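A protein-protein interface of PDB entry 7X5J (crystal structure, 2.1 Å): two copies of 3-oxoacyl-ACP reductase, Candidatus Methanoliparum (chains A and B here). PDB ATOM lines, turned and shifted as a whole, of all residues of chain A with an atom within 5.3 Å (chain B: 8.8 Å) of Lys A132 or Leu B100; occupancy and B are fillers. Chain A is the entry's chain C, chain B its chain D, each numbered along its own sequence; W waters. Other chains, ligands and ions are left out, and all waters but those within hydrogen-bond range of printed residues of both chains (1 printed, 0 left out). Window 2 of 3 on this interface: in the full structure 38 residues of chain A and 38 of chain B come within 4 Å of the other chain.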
ATOM      1  N   ILE A 128      23.717  -8.693  18.627  1.00  0.00           N
ATOM      2  CA  ILE A 128      23.118  -7.376  18.987  1.00  0.00           C
ATOM      3  C   ILE A 128      24.200  -6.296  19.115  1.00  0.00           C
ATOM      4  O   ILE A 128      23.933  -5.129  18.801  1.00  0.00           O
ATOM      5  CB  ILE A 128      22.184  -7.467  20.212  1.00  0.00           C
ATOM      6  CG1 ILE A 128      21.280  -6.232  20.292  1.00  0.00           C
ATOM      7  CG2 ILE A 128      22.952  -7.709  21.499  1.00  0.00           C
ATOM      8  CD1 ILE A 128      20.091  -6.370  21.220  1.00  0.00           C
ATOM      9  N   PRO A 129      25.441  -6.598  19.557  1.00  0.00           N
ATOM     10  CA  PRO A 129      26.476  -5.560  19.629  1.00  0.00           C
ATOM     11  C   PRO A 129      26.718  -4.886  18.265  1.00  0.00           C
ATOM     12  O   PRO A 129      26.711  -3.665  18.226  1.00  0.00           O
ATOM     13  CB  PRO A 129      27.706  -6.306  20.177  1.00  0.00           C
ATOM     14  CG  PRO A 129      27.097  -7.466  20.936  1.00  0.00           C
ATOM     15  CD  PRO A 129      25.928  -7.890  20.067  1.00  0.00           C
ATOM     16  N   ASP A 130      26.808  -5.654  17.177  1.00  0.00           N
ATOM     17  CA  ASP A 130      26.994  -5.105  15.806  1.00  0.00           C
ATOM     18  C   ASP A 130      25.710  -4.415  15.330  1.00  0.00           C
ATOM     19  O   ASP A 130      25.831  -3.414  14.624  1.00  0.00           O
ATOM     20  CB  ASP A 130      27.513  -6.160  14.824  1.00  0.00           C
ATOM     21  CG  ASP A 130      29.024  -6.295  14.920  1.00  0.00           C
ATOM     22  OD1 ASP A 130      29.626  -5.416  15.582  1.00  0.00           O
ATOM     23  OD2 ASP A 130      29.587  -7.272  14.358  1.00  0.00           O
ATOM     24  N   MET A 131      24.526  -4.897  15.711  1.00  0.00           N
ATOM     25  CA  MET A 131      23.247  -4.199  15.390  1.00  0.00           C
ATOM     26  C   MET A 131      23.246  -2.813  16.047  1.00  0.00           C
ATOM     27  O   MET A 131      22.892  -1.836  15.362  1.00  0.00           O
ATOM     28  CB  MET A 131      22.037  -4.987  15.894  1.00  0.00           C
ATOM     29  CG  MET A 131      21.707  -6.203  15.070  1.00  0.00           C
ATOM     30  SD  MET A 131      20.403  -7.173  15.907  1.00  0.00           S
ATOM     31  CE  MET A 131      20.204  -8.521  14.751  1.00  0.00           C
ATOM     32  N   LYS A 132      23.624  -2.724  17.326  1.00  0.00           N
ATOM     33  CA  LYS A 132      23.666  -1.429  18.069  1.00  0.00           C
ATOM     34  C   LYS A 132      24.663  -0.489  17.374  1.00  0.00           C
ATOM     35  O   LYS A 132      24.274   0.634  17.013  1.00  0.00           O
ATOM     36  CB  LYS A 132      24.066  -1.629  19.529  1.00  0.00           C
ATOM     37  CG  LYS A 132      23.004  -2.282  20.392  1.00  0.00           C
ATOM     38  CD  LYS A 132      23.429  -2.503  21.819  1.00  0.00           C
ATOM     39  CE  LYS A 132      22.274  -2.943  22.681  1.00  0.00           C
ATOM     40  NZ  LYS A 132      22.499  -2.643  24.110  1.00  0.00           N
ATOM     41  N   LYS A 133      25.882  -0.977  17.144  1.00  0.00           N
ATOM     42  CA  LYS A 133      26.983  -0.239  16.474  1.00  0.00           C
ATOM     43  C   LYS A 133      26.460   0.309  15.137  1.00  0.00           C
ATOM     44  O   LYS A 133      26.790   1.447  14.780  1.00  0.00           O
ATOM     45  CB  LYS A 133      28.181  -1.192  16.373  1.00  0.00           C
ATOM     46  CG  LYS A 133      29.382  -0.731  15.558  1.00  0.00           C
ATOM     47  CD  LYS A 133      30.211  -1.910  15.058  1.00  0.00           C
ATOM     48  CE  LYS A 133      31.678  -1.586  14.843  1.00  0.00           C
ATOM     49  NZ  LYS A 133      32.408  -1.446  16.128  1.00  0.00           N
ATOM     50  N   ASN A 134      25.615  -0.453  14.453  1.00  0.00           N
ATOM     51  CA  ASN A 134      25.102  -0.116  13.104  1.00  0.00           C
ATOM     52  C   ASN A 134      23.772   0.663  13.197  1.00  0.00           C
ATOM     53  O   ASN A 134      23.274   1.114  12.151  1.00  0.00           O
ATOM     54  CB  ASN A 134      25.011  -1.405  12.291  1.00  0.00           C
ATOM     55  CG  ASN A 134      25.065  -1.138  10.810  1.00  0.00           C
ATOM     56  OD1 ASN A 134      24.074  -0.725  10.207  1.00  0.00           O
ATOM     57  ND2 ASN A 134      26.231  -1.349  10.229  1.00  0.00           N
ATOM     58  N   ASN A 135      23.206   0.814  14.394  1.00  0.00           N
ATOM     59  CA  ASN A 135      21.904   1.501  14.641  1.00  0.00           C
ATOM     60  C   ASN A 135      20.798   0.929  13.742  1.00  0.00           C
ATOM     61  O   ASN A 135      19.963   1.705  13.257  1.00  0.00           O
ATOM     62  CB  ASN A 135      22.008   3.019  14.485  1.00  0.00           C
ATOM     63  CG  ASN A 135      22.112   3.691  15.832  1.00  0.00           C
ATOM     64  OD1 ASN A 135      21.106   4.013  16.459  1.00  0.00           O
ATOM     65  ND2 ASN A 135      23.328   3.874  16.308  1.00  0.00           N
ATOM     66  N   TRP A 136      20.782  -0.384  13.546  1.00  0.00           N
ATOM     67  CA  TRP A 136      19.675  -1.076  12.842  1.00  0.00           C
ATOM     68  C   TRP A 136      19.687  -2.560  13.210  1.00  0.00           C
ATOM     69  O   TRP A 136      20.752  -3.127  13.334  1.00  0.00           O
ATOM     70  CB  TRP A 136      19.779  -0.842  11.335  1.00  0.00           C
ATOM     71  CG  TRP A 136      18.504  -1.111  10.592  1.00  0.00           C
ATOM     72  CD1 TRP A 136      17.542  -0.207  10.236  1.00  0.00           C
ATOM     73  CD2 TRP A 136      18.034  -2.396  10.135  1.00  0.00           C
ATOM     74  NE1 TRP A 136      16.516  -0.834   9.572  1.00  0.00           N
ATOM     75  CE2 TRP A 136      16.794  -2.175   9.489  1.00  0.00           C
ATOM     76  CE3 TRP A 136      18.533  -3.703  10.219  1.00  0.00           C
ATOM     77  CZ2 TRP A 136      16.074  -3.211   8.893  1.00  0.00           C
ATOM     78  CZ3 TRP A 136      17.814  -4.724   9.639  1.00  0.00           C
ATOM     79  CH2 TRP A 136      16.602  -4.481   8.986  1.00  0.00           C
ATOM     80  N   GLU A 174      15.879  -2.894  25.348  1.00  0.00           N
ATOM     81  CA  GLU A 174      17.342  -2.648  25.220  1.00  0.00           C
ATOM     82  C   GLU A 174      17.679  -2.143  23.801  1.00  0.00           C
ATOM     83  O   GLU A 174      18.636  -1.360  23.685  1.00  0.00           O
ATOM     84  CB  GLU A 174      18.140  -3.895  25.620  1.00  0.00           C
ATOM     85  CG  GLU A 174      17.869  -4.353  27.056  1.00  0.00           C
ATOM     86  CD  GLU A 174      18.605  -5.617  27.495  1.00  0.00           C
ATOM     87  OE1 GLU A 174      19.442  -6.109  26.721  1.00  0.00           O
ATOM     88  OE2 GLU A 174      18.345  -6.100  28.620  1.00  0.00           O
ATOM     89  N   GLY A 175      16.919  -2.521  22.764  1.00  0.00           N
ATOM     90  CA  GLY A 175      17.291  -2.268  21.362  1.00  0.00           C
ATOM     91  C   GLY A 175      16.632  -1.036  20.758  1.00  0.00           C
ATOM     92  O   GLY A 175      17.074  -0.615  19.647  1.00  0.00           O
ATOM     93  N   TYR A 178      18.295   2.024  19.226  1.00  0.00           N
ATOM     94  CA  TYR A 178      19.237   1.618  18.153  1.00  0.00           C
ATOM     95  C   TYR A 178      18.523   1.256  16.847  1.00  0.00           C
ATOM     96  O   TYR A 178      19.195   0.709  15.983  1.00  0.00           O
ATOM     97  CB  TYR A 178      20.087   0.454  18.661  1.00  0.00           C
ATOM     98  CG  TYR A 178      20.874   0.866  19.874  1.00  0.00           C
ATOM     99  CD1 TYR A 178      22.071   1.554  19.745  1.00  0.00           C
ATOM    100  CD2 TYR A 178      20.359   0.688  21.144  1.00  0.00           C
ATOM    101  CE1 TYR A 178      22.770   1.993  20.853  1.00  0.00           C
ATOM    102  CE2 TYR A 178      21.048   1.110  22.266  1.00  0.00           C
ATOM    103  CZ  TYR A 178      22.252   1.773  22.117  1.00  0.00           C
ATOM    104  OH  TYR A 178      22.926   2.189  23.227  1.00  0.00           O
ATOM    105  N   ILE A 180      16.735  -1.169  16.651  1.00  0.00           N
ATOM    106  CA  ILE A 180      16.621  -2.656  16.753  1.00  0.00           C
ATOM    107  C   ILE A 180      15.207  -2.959  17.271  1.00  0.00           C
ATOM    108  O   ILE A 180      14.935  -2.628  18.450  1.00  0.00           O
ATOM    109  CB  ILE A 180      17.709  -3.265  17.661  1.00  0.00           C
ATOM    110  CG1 ILE A 180      19.124  -2.851  17.238  1.00  0.00           C
ATOM    111  CG2 ILE A 180      17.574  -4.782  17.692  1.00  0.00           C
ATOM    112  CD1 ILE A 180      20.180  -3.089  18.309  1.00  0.00           C
ATOM    113  N   ARG B  97      18.758  -8.680  38.657  1.00  0.00           N
ATOM    114  CA  ARG B  97      19.800  -8.421  37.634  1.00  0.00           C
ATOM    115  C   ARG B  97      19.509  -7.063  36.982  1.00  0.00           C
ATOM    116  O   ARG B  97      18.328  -6.652  36.927  1.00  0.00           O
ATOM    117  CB  ARG B  97      19.848  -9.537  36.595  1.00  0.00           C
ATOM    118  CG  ARG B  97      19.973 -10.919  37.212  1.00  0.00           C
ATOM    119  CD  ARG B  97      20.858 -11.820  36.388  1.00  0.00           C
ATOM    120  NE  ARG B  97      20.961 -13.131  37.010  1.00  0.00           N
ATOM    121  CZ  ARG B  97      21.658 -13.421  38.110  1.00  0.00           C
ATOM    122  NH1 ARG B  97      22.357 -12.493  38.745  1.00  0.00           N
ATOM    123  NH2 ARG B  97      21.674 -14.662  38.560  1.00  0.00           N
ATOM    124  N   ALA B  98      20.561  -6.365  36.570  1.00  0.00           N
ATOM    125  CA  ALA B  98      20.503  -5.100  35.807  1.00  0.00           C
ATOM    126  C   ALA B  98      21.670  -5.130  34.822  1.00  0.00           C
ATOM    127  O   ALA B  98      22.636  -4.397  35.018  1.00  0.00           O
ATOM    128  CB  ALA B  98      20.561  -3.923  36.746  1.00  0.00           C
ATOM    129  N   THR B  99      21.607  -6.045  33.860  1.00  0.00           N
ATOM    130  CA  THR B  99      22.704  -6.356  32.921  1.00  0.00           C
ATOM    131  C   THR B  99      22.093  -6.573  31.548  1.00  0.00           C
ATOM    132  O   THR B  99      21.238  -7.464  31.450  1.00  0.00           O
ATOM    133  CB  THR B  99      23.455  -7.603  33.394  1.00  0.00           C
ATOM    134  OG1 THR B  99      23.874  -7.296  34.722  1.00  0.00           O
ATOM    135  CG2 THR B  99      24.639  -7.970  32.529  1.00  0.00           C
ATOM    136  N   LEU B 100      22.476  -5.760  30.561  1.00  0.00           N
ATOM    137  CA  LEU B 100      21.988  -5.883  29.167  1.00  0.00           C
ATOM    138  C   LEU B 100      22.278  -7.311  28.723  1.00  0.00           C
ATOM    139  O   LEU B 100      23.212  -7.928  29.302  1.00  0.00           O
ATOM    140  CB  LEU B 100      22.687  -4.865  28.260  1.00  0.00           C
ATOM    141  CG  LEU B 100      22.468  -3.394  28.619  1.00  0.00           C
ATOM    142  CD1 LEU B 100      23.073  -2.493  27.557  1.00  0.00           C
ATOM    143  CD2 LEU B 100      20.986  -3.071  28.813  1.00  0.00           C
ATOM    144  N   ILE B 101      21.517  -7.815  27.748  1.00  0.00           N
ATOM    145  CA  ILE B 101      21.613  -9.243  27.326  1.00  0.00           C
ATOM    146  C   ILE B 101      23.050  -9.583  26.897  1.00  0.00           C
ATOM    147  O   ILE B 101      23.545 -10.648  27.338  1.00  0.00           O
ATOM    148  CB  ILE B 101      20.543  -9.605  26.269  1.00  0.00           C
ATOM    149  CG1 ILE B 101      20.610 -11.089  25.896  1.00  0.00           C
ATOM    150  CG2 ILE B 101      20.595  -8.695  25.045  1.00  0.00           C
ATOM    151  CD1 ILE B 101      19.325 -11.636  25.313  1.00  0.00           C
ATOM    152  N   GLU B 102      23.710  -8.733  26.101  1.00  0.00           N
ATOM    153  CA  GLU B 102      25.050  -9.052  25.527  1.00  0.00           C
ATOM    154  C   GLU B 102      26.097  -9.125  26.650  1.00  0.00           C
ATOM    155  O   GLU B 102      27.069  -9.868  26.471  1.00  0.00           O
ATOM    156  CB  GLU B 102      25.488  -8.067  24.434  1.00  0.00           C
ATOM    157  CG  GLU B 102      25.616  -6.632  24.917  1.00  0.00           C
ATOM    158  CD  GLU B 102      24.387  -5.777  24.667  1.00  0.00           C
ATOM    159  OE1 GLU B 102      23.263  -6.233  25.003  1.00  0.00           O
ATOM    160  OE2 GLU B 102      24.556  -4.679  24.119  1.00  0.00           O
ATOM    161  N   LYS B 103      25.889  -8.420  27.763  1.00  0.00           N
ATOM    162  CA  LYS B 103      26.805  -8.424  28.934  1.00  0.00           C
ATOM    163  C   LYS B 103      26.328  -9.421  30.002  1.00  0.00           C
ATOM    164  O   LYS B 103      26.926  -9.418  31.090  1.00  0.00           O
ATOM    165  CB  LYS B 103      26.883  -7.018  29.540  1.00  0.00           C
ATOM    166  CG  LYS B 103      27.648  -5.981  28.729  1.00  0.00           C
ATOM    167  CD  LYS B 103      29.092  -5.794  29.172  1.00  0.00           C
ATOM    168  CE  LYS B 103      29.446  -4.346  29.464  1.00  0.00           C
ATOM    169  NZ  LYS B 103      29.301  -3.487  28.262  1.00  0.00           N
ATOM    170  N   THR B 104      25.283 -10.219  29.739  1.00  0.00           N
ATOM    171  CA  THR B 104      24.713 -11.175  30.728  1.00  0.00           C
ATOM    172  C   THR B 104      25.451 -12.502  30.558  1.00  0.00           C
ATOM    173  O   THR B 104      25.527 -12.981  29.426  1.00  0.00           O
ATOM    174  CB  THR B 104      23.189 -11.338  30.593  1.00  0.00           C
ATOM    175  OG1 THR B 104      22.505 -10.103  30.845  1.00  0.00           O
ATOM    176  CG2 THR B 104      22.660 -12.410  31.519  1.00  0.00           C
ATOM    177  N   ALA B 105      25.995 -13.056  31.643  1.00  0.00           N
ATOM    178  CA  ALA B 105      26.791 -14.303  31.638  1.00  0.00           C
ATOM    179  C   ALA B 105      25.861 -15.512  31.475  1.00  0.00           C
ATOM    180  O   ALA B 105      24.844 -15.587  32.185  1.00  0.00           O
ATOM    181  CB  ALA B 105      27.582 -14.397  32.915  1.00  0.00           C
ATOM    182  N   GLY B 151      11.577  -5.935  30.839  1.00  0.00           N
ATOM    183  CA  GLY B 151      12.357  -5.008  31.680  1.00  0.00           C
ATOM    184  C   GLY B 151      13.800  -4.936  31.222  1.00  0.00           C
ATOM    185  O   GLY B 151      14.461  -6.006  31.089  1.00  0.00           O
ATOM    186  N   SER B 152      14.298  -3.733  30.955  1.00  0.00           N
ATOM    187  CA  SER B 152      15.683  -3.551  30.451  1.00  0.00           C
ATOM    188  C   SER B 152      16.642  -4.177  31.469  1.00  0.00           C
ATOM    189  O   SER B 152      16.430  -3.965  32.646  1.00  0.00           O
ATOM    190  CB  SER B 152      15.995  -2.103  30.167  1.00  0.00           C
ATOM    191  OG  SER B 152      17.313  -1.984  29.648  1.00  0.00           O
ATOM    192  N   GLY B 153      17.600  -4.985  31.012  1.00  0.00           N
ATOM    193  CA  GLY B 153      18.674  -5.570  31.840  1.00  0.00           C
ATOM    194  C   GLY B 153      18.198  -6.768  32.637  1.00  0.00           C
ATOM    195  O   GLY B 153      18.962  -7.250  33.496  1.00  0.00           O
ATOM    196  N   GLN B 154      17.012  -7.289  32.313  1.00  0.00           N
ATOM    197  CA  GLN B 154      16.397  -8.427  33.031  1.00  0.00           C
ATOM    198  C   GLN B 154      15.994  -9.539  32.063  1.00  0.00           C
ATOM    199  O   GLN B 154      14.871 -10.038  32.210  1.00  0.00           O
ATOM    200  CB  GLN B 154      15.178  -7.910  33.787  1.00  0.00           C
ATOM    201  CG  GLN B 154      15.496  -6.762  34.723  1.00  0.00           C
ATOM    202  CD  GLN B 154      14.537  -6.778  35.884  1.00  0.00           C
ATOM    203  OE1 GLN B 154      13.683  -5.899  36.022  1.00  0.00           O
ATOM    204  NE2 GLN B 154      14.641  -7.815  36.706  1.00  0.00           N
ATOM    205  N   CYS B 155      16.871  -9.975  31.156  1.00  0.00           N
ATOM    206  CA  CYS B 155      16.479 -10.918  30.082  1.00  0.00           C
ATOM    207  C   CYS B 155      16.037 -12.272  30.681  1.00  0.00           C
ATOM    208  O   CYS B 155      15.048 -12.857  30.181  1.00  0.00           O
ATOM    209  CB  CYS B 155      17.565 -11.050  29.024  1.00  0.00           C
ATOM    210  SG  CYS B 155      19.137 -11.719  29.625  1.00  0.00           S
ATOM    211  N   SER B 156      16.704 -12.763  31.726  1.00  0.00           N
ATOM    212  CA  SER B 156      16.421 -14.084  32.342  1.00  0.00           C
ATOM    213  C   SER B 156      15.149 -13.992  33.189  1.00  0.00           C
ATOM    214  O   SER B 156      14.365 -14.971  33.230  1.00  0.00           O
ATOM    215  CB  SER B 156      17.569 -14.549  33.193  1.00  0.00           C
ATOM    216  OG  SER B 156      17.496 -13.957  34.491  1.00  0.00           O
HETATM  217  O   HOH W   1      20.850  -5.055  24.796  1.00  0.00           O
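OE1 of Glu A174 is in hydrogen-bond range of N of Ile B101 (2.9 Å). OE2 of Glu B102 is in salt-bridge range of NZ of Lys A132 (2.9 Å). OE2 of Glu A174 lies within hydrogen-bond range of N of Gly B153 (2.7 Å).
N of Thr B99 lies within hydrogen-bond range of O of Gly B153, at 2.9 Å. The side-chain hydroxyl (OG1) of Thr B104 sits at hydrogen-bond distance from the backbone carbonyl oxygen (O) of Leu B100 (2.8 Å). The side-chain amide nitrogen of Asn A135 is in hydrogen-bond range of the backbone carbonyl oxygen of Lys A132, 3.4 Å away.
Ile A128 touches Glu B102 (CG2 to OE1, 3.8 Å). Glu B102 touches Pro A129 (CB to CG, 3.9 Å). Lys A132 touches Leu B100 (NZ to CD1, 3.5 Å). Leu B100 touches Glu A174 (CA to OE1, 3.5 Å). OG of Ser B152 touches CG of Glu A174 (3.6 Å).
Printed residues of chain B within 4 Å of Ile A128: Glu B102 (3.8 Å). Of the printed residues of chain B, Lys A132 touches Leu B100 (3.5 Å) and Glu B102 (2.9 Å). Of the printed residues of chain B, Glu A174 touches Leu B100, Ile B101, Ser B152 and Gly B153. Leu B100 touches just these residues of chain A: Lys A132 and Glu A174. Of the printed residues of chain A, Ile B101 touches Glu A174 (2.9 Å). Of the printed residues of chain A, Glu B102 touches Ile A128, Pro A129 and Lys A132. Printed residues of chain A within 4 Å of Gly B153: Glu A174 (2.7 Å). The nearest residue of chain B that does not touch Lys A132 is Ile B101 (6.4 Å). The nearest printed residue of chain A that does not touch Leu B100 is Tyr A178 (6.4 Å).
Printed residues of chain B that touch a printed residue of chain A: Leu B100, Ile B101, Glu B102, Ser B152 and Gly B153. Among the printed residues, 8 pairs touch across the chains. Among the printed residues, Asp or Glu carboxylates within 4 Å of a Lys or Arg side-chain nitrogen of the other chain: Lys A132 with Glu B102 (2.9 Å).
No position is printed for both chains.
Water W1 lies within hydrogen-bond range of the side-chain carboxylate (OE1) of Glu A174, the side-chain carboxylate (OE1) of Glu B102 and the side-chain amino group (NZ) of Lys A132.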
